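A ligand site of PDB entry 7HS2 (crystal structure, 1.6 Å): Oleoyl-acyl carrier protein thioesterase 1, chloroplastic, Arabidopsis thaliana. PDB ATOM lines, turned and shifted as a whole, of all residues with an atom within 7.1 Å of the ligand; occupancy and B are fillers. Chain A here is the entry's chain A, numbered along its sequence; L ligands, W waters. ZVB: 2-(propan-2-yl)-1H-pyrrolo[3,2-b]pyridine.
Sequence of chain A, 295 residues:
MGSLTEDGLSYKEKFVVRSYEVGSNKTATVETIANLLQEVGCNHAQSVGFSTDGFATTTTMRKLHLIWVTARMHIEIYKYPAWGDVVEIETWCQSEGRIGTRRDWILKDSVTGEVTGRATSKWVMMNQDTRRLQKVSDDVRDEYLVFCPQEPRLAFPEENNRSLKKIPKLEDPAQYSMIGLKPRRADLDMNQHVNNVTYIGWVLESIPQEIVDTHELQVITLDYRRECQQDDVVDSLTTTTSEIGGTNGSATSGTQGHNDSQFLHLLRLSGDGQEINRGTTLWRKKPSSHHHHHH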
ATOM      1  N   TRP A  68     -20.182  -2.745  12.203  1.00  0.00           N
ATOM      2  CA  TRP A  68     -19.880  -3.671  13.295  1.00  0.00           C
ATOM      3  C   TRP A  68     -20.337  -3.044  14.584  1.00  0.00           C
ATOM      4  O   TRP A  68     -20.169  -1.828  14.774  1.00  0.00           O
ATOM      5  CB  TRP A  68     -18.367  -3.919  13.435  1.00  0.00           C
ATOM      6  CG  TRP A  68     -17.722  -4.602  12.287  1.00  0.00           C
ATOM      7  CD1 TRP A  68     -16.805  -4.071  11.431  1.00  0.00           C
ATOM      8  CD2 TRP A  68     -17.855  -5.986  11.928  1.00  0.00           C
ATOM      9  NE1 TRP A  68     -16.383  -5.030  10.546  1.00  0.00           N
ATOM     10  CE2 TRP A  68     -17.017  -6.211  10.826  1.00  0.00           C
ATOM     11  CE3 TRP A  68     -18.619  -7.055  12.435  1.00  0.00           C
ATOM     12  CZ2 TRP A  68     -16.918  -7.454  10.210  1.00  0.00           C
ATOM     13  CZ3 TRP A  68     -18.527  -8.286  11.816  1.00  0.00           C
ATOM     14  CH2 TRP A  68     -17.700  -8.467  10.702  1.00  0.00           C
ATOM     15  N   VAL A  69     -20.884  -3.864  15.485  1.00  0.00           N
ATOM     16  CA  VAL A  69     -21.231  -3.418  16.837  1.00  0.00           C
ATOM     17  C   VAL A  69     -20.610  -4.390  17.830  1.00  0.00           C
ATOM     18  O   VAL A  69     -20.537  -5.603  17.538  1.00  0.00           O
ATOM     19  CB  VAL A  69     -22.747  -3.203  17.109  1.00  0.00           C
ATOM     20  CG1 VAL A  69     -23.340  -2.130  16.196  1.00  0.00           C
ATOM     21  CG2 VAL A  69     -23.523  -4.501  17.020  1.00  0.00           C
ATOM     22  N   THR A  70     -20.149  -3.885  18.994  1.00  0.00           N
ATOM     23  CA  THR A  70     -19.561  -4.783  19.991  1.00  0.00           C
ATOM     24  C   THR A  70     -20.630  -5.628  20.632  1.00  0.00           C
ATOM     25  O   THR A  70     -21.676  -5.126  21.033  1.00  0.00           O
ATOM     26  CB  THR A  70     -18.806  -4.003  21.109  1.00  0.00           C
ATOM     27  OG1 THR A  70     -17.978  -2.998  20.548  1.00  0.00           O
ATOM     28  CG2 THR A  70     -17.969  -4.926  21.973  1.00  0.00           C
ATOM     29  N   ALA A  71     -20.392  -6.931  20.737  1.00  0.00           N
ATOM     30  CA  ALA A  71     -21.274  -7.826  21.466  1.00  0.00           C
ATOM     31  C   ALA A  71     -20.676  -8.052  22.893  1.00  0.00           C
ATOM     32  O   ALA A  71     -21.422  -8.227  23.844  1.00  0.00           O
ATOM     33  CB  ALA A  71     -21.398  -9.174  20.740  1.00  0.00           C
ATOM     34  N   ARG A  72     -19.334  -8.126  23.012  1.00  0.00           N
ATOM     35  CA  ARG A  72     -18.692  -8.393  24.303  1.00  0.00           C
ATOM     36  C   ARG A  72     -17.299  -7.805  24.322  1.00  0.00           C
ATOM     37  O   ARG A  72     -16.589  -7.843  23.322  1.00  0.00           O
ATOM     38  CB  ARG A  72     -18.614  -9.918  24.580  1.00  0.00           C
ATOM     39  CG  ARG A  72     -17.768 -10.265  25.835  1.00  0.00           C
ATOM     40  CD  ARG A  72     -17.780 -11.726  26.180  1.00  0.00           C
ATOM     41  NE  ARG A  72     -19.038 -12.063  26.814  1.00  0.00           N
ATOM     42  CZ  ARG A  72     -19.244 -13.157  27.547  1.00  0.00           C
ATOM     43  NH1 ARG A  72     -18.253 -14.012  27.777  1.00  0.00           N
ATOM     44  NH2 ARG A  72     -20.439 -13.390  28.082  1.00  0.00           N
ATOM     45  N   TRP A 123     -17.422  -8.897  17.884  1.00  0.00           N
ATOM     46  CA  TRP A 123     -18.166  -7.923  17.112  1.00  0.00           C
ATOM     47  C   TRP A 123     -19.143  -8.679  16.201  1.00  0.00           C
ATOM     48  O   TRP A 123     -18.814  -9.757  15.702  1.00  0.00           O
ATOM     49  CB  TRP A 123     -17.199  -7.074  16.251  1.00  0.00           C
ATOM     50  CG  TRP A 123     -16.191  -6.290  17.058  1.00  0.00           C
ATOM     51  CD1 TRP A 123     -15.084  -6.775  17.685  1.00  0.00           C
ATOM     52  CD2 TRP A 123     -16.267  -4.901  17.403  1.00  0.00           C
ATOM     53  NE1 TRP A 123     -14.452  -5.765  18.377  1.00  0.00           N
ATOM     54  CE2 TRP A 123     -15.151  -4.605  18.209  1.00  0.00           C
ATOM     55  CE3 TRP A 123     -17.173  -3.876  17.097  1.00  0.00           C
ATOM     56  CZ2 TRP A 123     -14.904  -3.317  18.689  1.00  0.00           C
ATOM     57  CZ3 TRP A 123     -16.896  -2.586  17.524  1.00  0.00           C
ATOM     58  CH2 TRP A 123     -15.776  -2.319  18.309  1.00  0.00           C
ATOM     59  N   VAL A 124     -20.363  -8.141  16.059  1.00  0.00           N
ATOM     60  CA  VAL A 124     -21.377  -8.736  15.197  1.00  0.00           C
ATOM     61  C   VAL A 124     -21.798  -7.707  14.121  1.00  0.00           C
ATOM     62  O   VAL A 124     -21.742  -6.493  14.354  1.00  0.00           O
ATOM     63  CB  VAL A 124     -22.593  -9.286  15.984  1.00  0.00           C
ATOM     64  CG1 VAL A 124     -22.139 -10.423  16.895  1.00  0.00           C
ATOM     65  CG2 VAL A 124     -23.267  -8.180  16.794  1.00  0.00           C
ATOM     66  N   MET A 126     -24.328  -5.583  11.730  1.00  0.00           N
ATOM     67  CA  MET A 126     -25.671  -5.027  11.842  1.00  0.00           C
ATOM     68  C   MET A 126     -25.959  -4.142  10.635  1.00  0.00           C
ATOM     69  O   MET A 126     -25.052  -3.455  10.138  1.00  0.00           O
ATOM     70  CB  MET A 126     -25.719  -4.142  13.117  1.00  0.00           C
ATOM     71  CG  MET A 126     -27.027  -3.408  13.328  1.00  0.00           C
ATOM     72  SD  MET A 126     -26.968  -2.252  14.714  1.00  0.00           S
ATOM     73  CE  MET A 126     -27.100  -3.410  16.079  1.00  0.00           C
ATOM     74  N   ARG A 131     -31.069  -1.697  12.092  1.00  0.00           N
ATOM     75  CA  ARG A 131     -30.463  -2.168  13.336  1.00  0.00           C
ATOM     76  C   ARG A 131     -30.590  -3.697  13.494  1.00  0.00           C
ATOM     77  O   ARG A 131     -30.491  -4.198  14.612  1.00  0.00           O
ATOM     78  CB  ARG A 131     -30.986  -1.406  14.566  1.00  0.00           C
ATOM     79  CG  ARG A 131     -30.810   0.114  14.447  1.00  0.00           C
ATOM     80  CD  ARG A 131     -29.363   0.543  14.486  1.00  0.00           C
ATOM     81  NE  ARG A 131     -28.780   0.358  15.824  1.00  0.00           N
ATOM     82  CZ  ARG A 131     -27.551   0.700  16.162  1.00  0.00           C
ATOM     83  NH1 ARG A 131     -27.109   0.452  17.390  1.00  0.00           N
ATOM     84  NH2 ARG A 131     -26.746   1.305  15.291  1.00  0.00           N
ATOM     85  N   LEU A 133     -29.349  -7.506  13.253  1.00  0.00           N
ATOM     86  CA  LEU A 133     -28.100  -8.279  13.189  1.00  0.00           C
ATOM     87  C   LEU A 133     -28.128  -9.272  12.049  1.00  0.00           C
ATOM     88  O   LEU A 133     -29.191  -9.736  11.648  1.00  0.00           O
ATOM     89  CB  LEU A 133     -27.899  -9.075  14.497  1.00  0.00           C
ATOM     90  CG  LEU A 133     -27.825  -8.233  15.772  1.00  0.00           C
ATOM     91  CD1 LEU A 133     -27.583  -9.141  16.950  1.00  0.00           C
ATOM     92  CD2 LEU A 133     -26.691  -7.180  15.691  1.00  0.00           C
ATOM     93  N   HIS A 193     -23.093   8.672  18.603  1.00  0.00           N
ATOM     94  CA  HIS A 193     -23.529   7.492  19.341  1.00  0.00           C
ATOM     95  C   HIS A 193     -22.757   7.469  20.673  1.00  0.00           C
ATOM     96  O   HIS A 193     -21.598   7.890  20.702  1.00  0.00           O
ATOM     97  CB  HIS A 193     -23.208   6.199  18.569  1.00  0.00           C
ATOM     98  CG  HIS A 193     -24.064   6.007  17.353  1.00  0.00           C
ATOM     99  ND1 HIS A 193     -25.233   5.276  17.398  1.00  0.00           N
ATOM    100  CD2 HIS A 193     -23.901   6.493  16.097  1.00  0.00           C
ATOM    101  CE1 HIS A 193     -25.759   5.350  16.182  1.00  0.00           C
ATOM    102  NE2 HIS A 193     -25.000   6.066  15.364  1.00  0.00           N
ATOM    103  N   VAL A 194     -23.343   6.920  21.736  1.00  0.00           N
ATOM    104  CA  VAL A 194     -22.632   6.778  23.007  1.00  0.00           C
ATOM    105  C   VAL A 194     -21.392   5.877  22.825  1.00  0.00           C
ATOM    106  O   VAL A 194     -21.509   4.784  22.276  1.00  0.00           O
ATOM    107  CB  VAL A 194     -23.532   6.286  24.160  1.00  0.00           C
ATOM    108  CG1 VAL A 194     -22.707   6.061  25.435  1.00  0.00           C
ATOM    109  CG2 VAL A 194     -24.667   7.289  24.419  1.00  0.00           C
ATOM    110  N   ASN A 196     -18.559   3.188  23.402  1.00  0.00           N
ATOM    111  CA  ASN A 196     -18.600   1.923  24.143  1.00  0.00           C
ATOM    112  C   ASN A 196     -17.991   2.002  25.550  1.00  0.00           C
ATOM    113  O   ASN A 196     -18.371   1.207  26.418  1.00  0.00           O
ATOM    114  CB  ASN A 196     -17.824   0.837  23.415  1.00  0.00           C
ATOM    115  CG  ASN A 196     -18.400   0.453  22.087  1.00  0.00           C
ATOM    116  OD1 ASN A 196     -19.614   0.438  21.903  1.00  0.00           O
ATOM    117  ND2 ASN A 196     -17.512   0.176  21.150  1.00  0.00           N
ATOM    118  N   TYR A 199     -20.241   2.881  28.721  1.00  0.00           N
ATOM    119  CA  TYR A 199     -20.995   1.794  29.401  1.00  0.00           C
ATOM    120  C   TYR A 199     -20.132   1.146  30.515  1.00  0.00           C
ATOM    121  O   TYR A 199     -20.661   0.785  31.557  1.00  0.00           O
ATOM    122  CB  TYR A 199     -21.406   0.740  28.404  1.00  0.00           C
ATOM    123  CG  TYR A 199     -22.301   1.279  27.303  1.00  0.00           C
ATOM    124  CD1 TYR A 199     -21.764   1.737  26.099  1.00  0.00           C
ATOM    125  CD2 TYR A 199     -23.681   1.271  27.431  1.00  0.00           C
ATOM    126  CE1 TYR A 199     -22.590   2.171  25.060  1.00  0.00           C
ATOM    127  CE2 TYR A 199     -24.507   1.763  26.418  1.00  0.00           C
ATOM    128  CZ  TYR A 199     -23.958   2.188  25.226  1.00  0.00           C
ATOM    129  OH  TYR A 199     -24.789   2.608  24.227  1.00  0.00           O
ATOM    130  N   ASP A 223     -21.204  -7.703  28.327  1.00  0.00           N
ATOM    131  CA  ASP A 223     -22.021  -8.006  27.161  1.00  0.00           C
ATOM    132  C   ASP A 223     -22.798  -6.738  26.811  1.00  0.00           C
ATOM    133  O   ASP A 223     -23.327  -6.064  27.724  1.00  0.00           O
ATOM    134  CB  ASP A 223     -23.062  -9.093  27.478  1.00  0.00           C
ATOM    135  CG  ASP A 223     -22.517 -10.499  27.552  1.00  0.00           C
ATOM    136  OD1 ASP A 223     -21.407 -10.723  27.031  1.00  0.00           O
ATOM    137  OD2 ASP A 223     -23.201 -11.361  28.132  1.00  0.00           O
ATOM    138  N   TYR A 224     -22.895  -6.412  25.524  1.00  0.00           N
ATOM    139  CA  TYR A 224     -23.618  -5.228  25.050  1.00  0.00           C
ATOM    140  C   TYR A 224     -24.839  -5.778  24.274  1.00  0.00           C
ATOM    141  O   TYR A 224     -24.679  -6.639  23.416  1.00  0.00           O
ATOM    142  CB  TYR A 224     -22.717  -4.376  24.133  1.00  0.00           C
ATOM    143  CG  TYR A 224     -21.557  -3.678  24.809  1.00  0.00           C
ATOM    144  CD1 TYR A 224     -20.426  -4.385  25.218  1.00  0.00           C
ATOM    145  CD2 TYR A 224     -21.513  -2.297  24.909  1.00  0.00           C
ATOM    146  CE1 TYR A 224     -19.322  -3.730  25.796  1.00  0.00           C
ATOM    147  CE2 TYR A 224     -20.424  -1.629  25.472  1.00  0.00           C
ATOM    148  CZ  TYR A 224     -19.331  -2.356  25.919  1.00  0.00           C
ATOM    149  OH  TYR A 224     -18.262  -1.654  26.465  1.00  0.00           O
ATOM    150  N   ARG A 225     -26.045  -5.342  24.612  1.00  0.00           N
ATOM    151  CA  ARG A 225     -27.287  -5.901  24.042  1.00  0.00           C
ATOM    152  C   ARG A 225     -28.097  -4.876  23.237  1.00  0.00           C
ATOM    153  O   ARG A 225     -28.819  -5.222  22.297  1.00  0.00           O
ATOM    154  CB  ARG A 225     -28.158  -6.351  25.251  1.00  0.00           C
ATOM    155  CG  ARG A 225     -29.431  -7.094  24.926  1.00  0.00           C
ATOM    156  CD  ARG A 225     -30.139  -7.500  26.209  1.00  0.00           C
ATOM    157  NE  ARG A 225     -31.146  -8.538  26.006  1.00  0.00           N
ATOM    158  CZ  ARG A 225     -30.975  -9.822  26.301  1.00  0.00           C
ATOM    159  NH1 ARG A 225     -29.801 -10.256  26.764  1.00  0.00           N
ATOM    160  NH2 ARG A 225     -31.956 -10.691  26.098  1.00  0.00           N
ATOM    161  N   ARG A 226     -28.015  -3.613  23.655  1.00  0.00           N
ATOM    162  CA  ARG A 226     -28.786  -2.526  23.093  1.00  0.00           C
ATOM    163  C   ARG A 226     -28.065  -1.208  23.345  1.00  0.00           C
ATOM    164  O   ARG A 226     -27.371  -1.055  24.338  1.00  0.00           O
ATOM    165  CB  ARG A 226     -30.123  -2.481  23.839  1.00  0.00           C
ATOM    166  CG  ARG A 226     -31.110  -1.458  23.343  1.00  0.00           C
ATOM    167  CD  ARG A 226     -32.487  -1.735  23.915  1.00  0.00           C
ATOM    168  NE  ARG A 226     -32.928  -3.116  23.667  1.00  0.00           N
ATOM    169  CZ  ARG A 226     -33.586  -3.516  22.586  1.00  0.00           C
ATOM    170  NH1 ARG A 226     -33.940  -4.786  22.441  1.00  0.00           N
ATOM    171  NH2 ARG A 226     -33.892  -2.654  21.628  1.00  0.00           N
ATOM    172  N   GLU A 227     -28.243  -0.265  22.449  1.00  0.00           N
ATOM    173  CA  GLU A 227     -27.629   1.041  22.544  1.00  0.00           C
ATOM    174  C   GLU A 227     -28.387   2.000  23.496  1.00  0.00           C
ATOM    175  O   GLU A 227     -29.624   1.996  23.528  1.00  0.00           O
ATOM    176  CB  GLU A 227     -27.610   1.620  21.133  1.00  0.00           C
ATOM    177  CG  GLU A 227     -27.027   2.995  20.984  1.00  0.00           C
ATOM    178  CD  GLU A 227     -26.598   3.266  19.557  1.00  0.00           C
ATOM    179  OE1 GLU A 227     -27.468   3.235  18.656  1.00  0.00           O
ATOM    180  OE2 GLU A 227     -25.379   3.493  19.340  1.00  0.00           O
ATOM    181  N   CYS A 228     -27.652   2.808  24.267  1.00  0.00           N
ATOM    182  CA  CYS A 228     -28.275   3.860  25.061  1.00  0.00           C
ATOM    183  C   CYS A 228     -28.319   5.065  24.114  1.00  0.00           C
ATOM    184  O   CYS A 228     -27.257   5.473  23.604  1.00  0.00           O
ATOM    185  CB  CYS A 228     -27.454   4.193  26.316  1.00  0.00           C
ATOM    186  SG  CYS A 228     -27.997   5.695  27.167  1.00  0.00           S
ATOM    187  N   ILE A 276     -29.663  -3.027  28.720  1.00  0.00           N
ATOM    188  CA  ILE A 276     -28.737  -2.561  27.692  1.00  0.00           C
ATOM    189  C   ILE A 276     -27.386  -3.323  27.795  1.00  0.00           C
ATOM    190  O   ILE A 276     -26.737  -3.544  26.772  1.00  0.00           O
ATOM    191  CB  ILE A 276     -28.556  -1.040  27.650  1.00  0.00           C
ATOM    192  CG1 ILE A 276     -27.949  -0.512  28.922  1.00  0.00           C
ATOM    193  CG2 ILE A 276     -29.885  -0.273  27.278  1.00  0.00           C
ATOM    194  CD1 ILE A 276     -27.456   0.962  28.800  1.00  0.00           C
ATOM    195  N   ASN A 277     -26.958  -3.721  29.030  1.00  0.00           N
ATOM    196  CA  ASN A 277     -25.717  -4.473  29.263  1.00  0.00           C
ATOM    197  C   ASN A 277     -25.842  -5.355  30.488  1.00  0.00           C
ATOM    198  O   ASN A 277     -26.590  -5.021  31.417  1.00  0.00           O
ATOM    199  CB  ASN A 277     -24.528  -3.512  29.614  1.00  0.00           C
ATOM    200  CG  ASN A 277     -24.199  -2.519  28.557  1.00  0.00           C
ATOM    201  OD1 ASN A 277     -24.916  -1.534  28.426  1.00  0.00           O
ATOM    202  ND2 ASN A 277     -23.138  -2.759  27.750  1.00  0.00           N
HETATM  203  N1  ZVB L   1     -27.354  -4.298  19.467  1.00  0.00           N
HETATM  204  C4  ZVB L   1     -24.656  -2.353  20.780  1.00  0.00           C
HETATM  205  C5  ZVB L   1     -25.924  -2.400  20.285  1.00  0.00           C
HETATM  206  C6  ZVB L   1     -26.230  -3.752  20.003  1.00  0.00           C
HETATM  207  C7  ZVB L   1     -27.340  -5.629  19.316  1.00  0.00           C
HETATM  208  C8  ZVB L   1     -26.247  -6.435  19.641  1.00  0.00           C
HETATM  209  C10 ZVB L   1     -25.106  -4.510  20.321  1.00  0.00           C
HETATM  210  C1  ZVB L   1     -22.361  -1.515  21.405  1.00  0.00           C
HETATM  211  C2  ZVB L   1     -23.844  -1.181  21.281  1.00  0.00           C
HETATM  212  C3  ZVB L   1     -24.032   0.036  20.377  1.00  0.00           C
HETATM  213  C9  ZVB L   1     -25.078  -5.891  20.140  1.00  0.00           C
HETATM  214  N2  ZVB L   1     -24.168  -3.646  20.818  1.00  0.00           N
HETATM  215  O   HOH W   1     -29.590  -7.466  21.264  1.00  0.00           O
HETATM  216  O   HOH W   2     -19.888  -0.971  19.194  1.00  0.00           O
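A nitrogen (N2) of the ligand sits at hydrogen-bond distance from the backbone carbonyl oxygen (O) of Thr 70, 2.9 Å away.
The backbone carbonyl oxygen (O) of Arg 225 sits close to a nitrogen (N1) of the ligand, at 3.3 Å.
The side-chain amide nitrogen (ND2) of Asn 196 lies within hydrogen-bond range of the side-chain hydroxyl (OG1) of Thr 70, 3.3 Å away.
The backbone NH of Arg 225 sits at hydrogen-bond distance from the backbone carbonyl oxygen of Ile 276 (2.9 Å).
The backbone carbonyl oxygen of Asn 196 lies within hydrogen-bond range of the side-chain hydroxyl of Tyr 224 (2.9 Å).
The backbone NH (N) of Tyr 224 lies within hydrogen-bond range of the backbone carbonyl oxygen (O) of Ala 71.
SD of Met 126 lies close to NE of Arg 131, 3.4 Å away.
The backbone carbonyl oxygen (O) of Val 69 lies within hydrogen-bond range of the backbone NH (N) of Val 124 (2.9 Å).
The guanidinium group of Arg 131 lies within salt-bridge range of the side-chain carboxylate of Glu 227 (3.1 Å).
A ring nitrogen (ND1) of His 193 is in hydrogen-bond range of the side-chain carboxylate of Glu 227, at 2.6 Å.
Merely in contact with the ligand: Tyr 224 (3.4 Å), Asn 196 (3.4 Å), Met 126 (3.5 Å), Val 69 (3.7 Å), Glu 227 (3.8 Å), Arg 226 (3.9 Å) and Leu 133 (3.996 Å).
Hydrophobic or aromatic side chains that line the ligand: Val 69, Met 126, Leu 133 and Tyr 224.
Of the 22 residues printed, 9 come within 4 Å of the ligand.
Along chain A the residues within 4 Å of the ligand span positions 69 to 227.
Water W2 bridges N of Thr 70 (2.9 Å) and OD1 of Asn 196 (3.1 Å).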
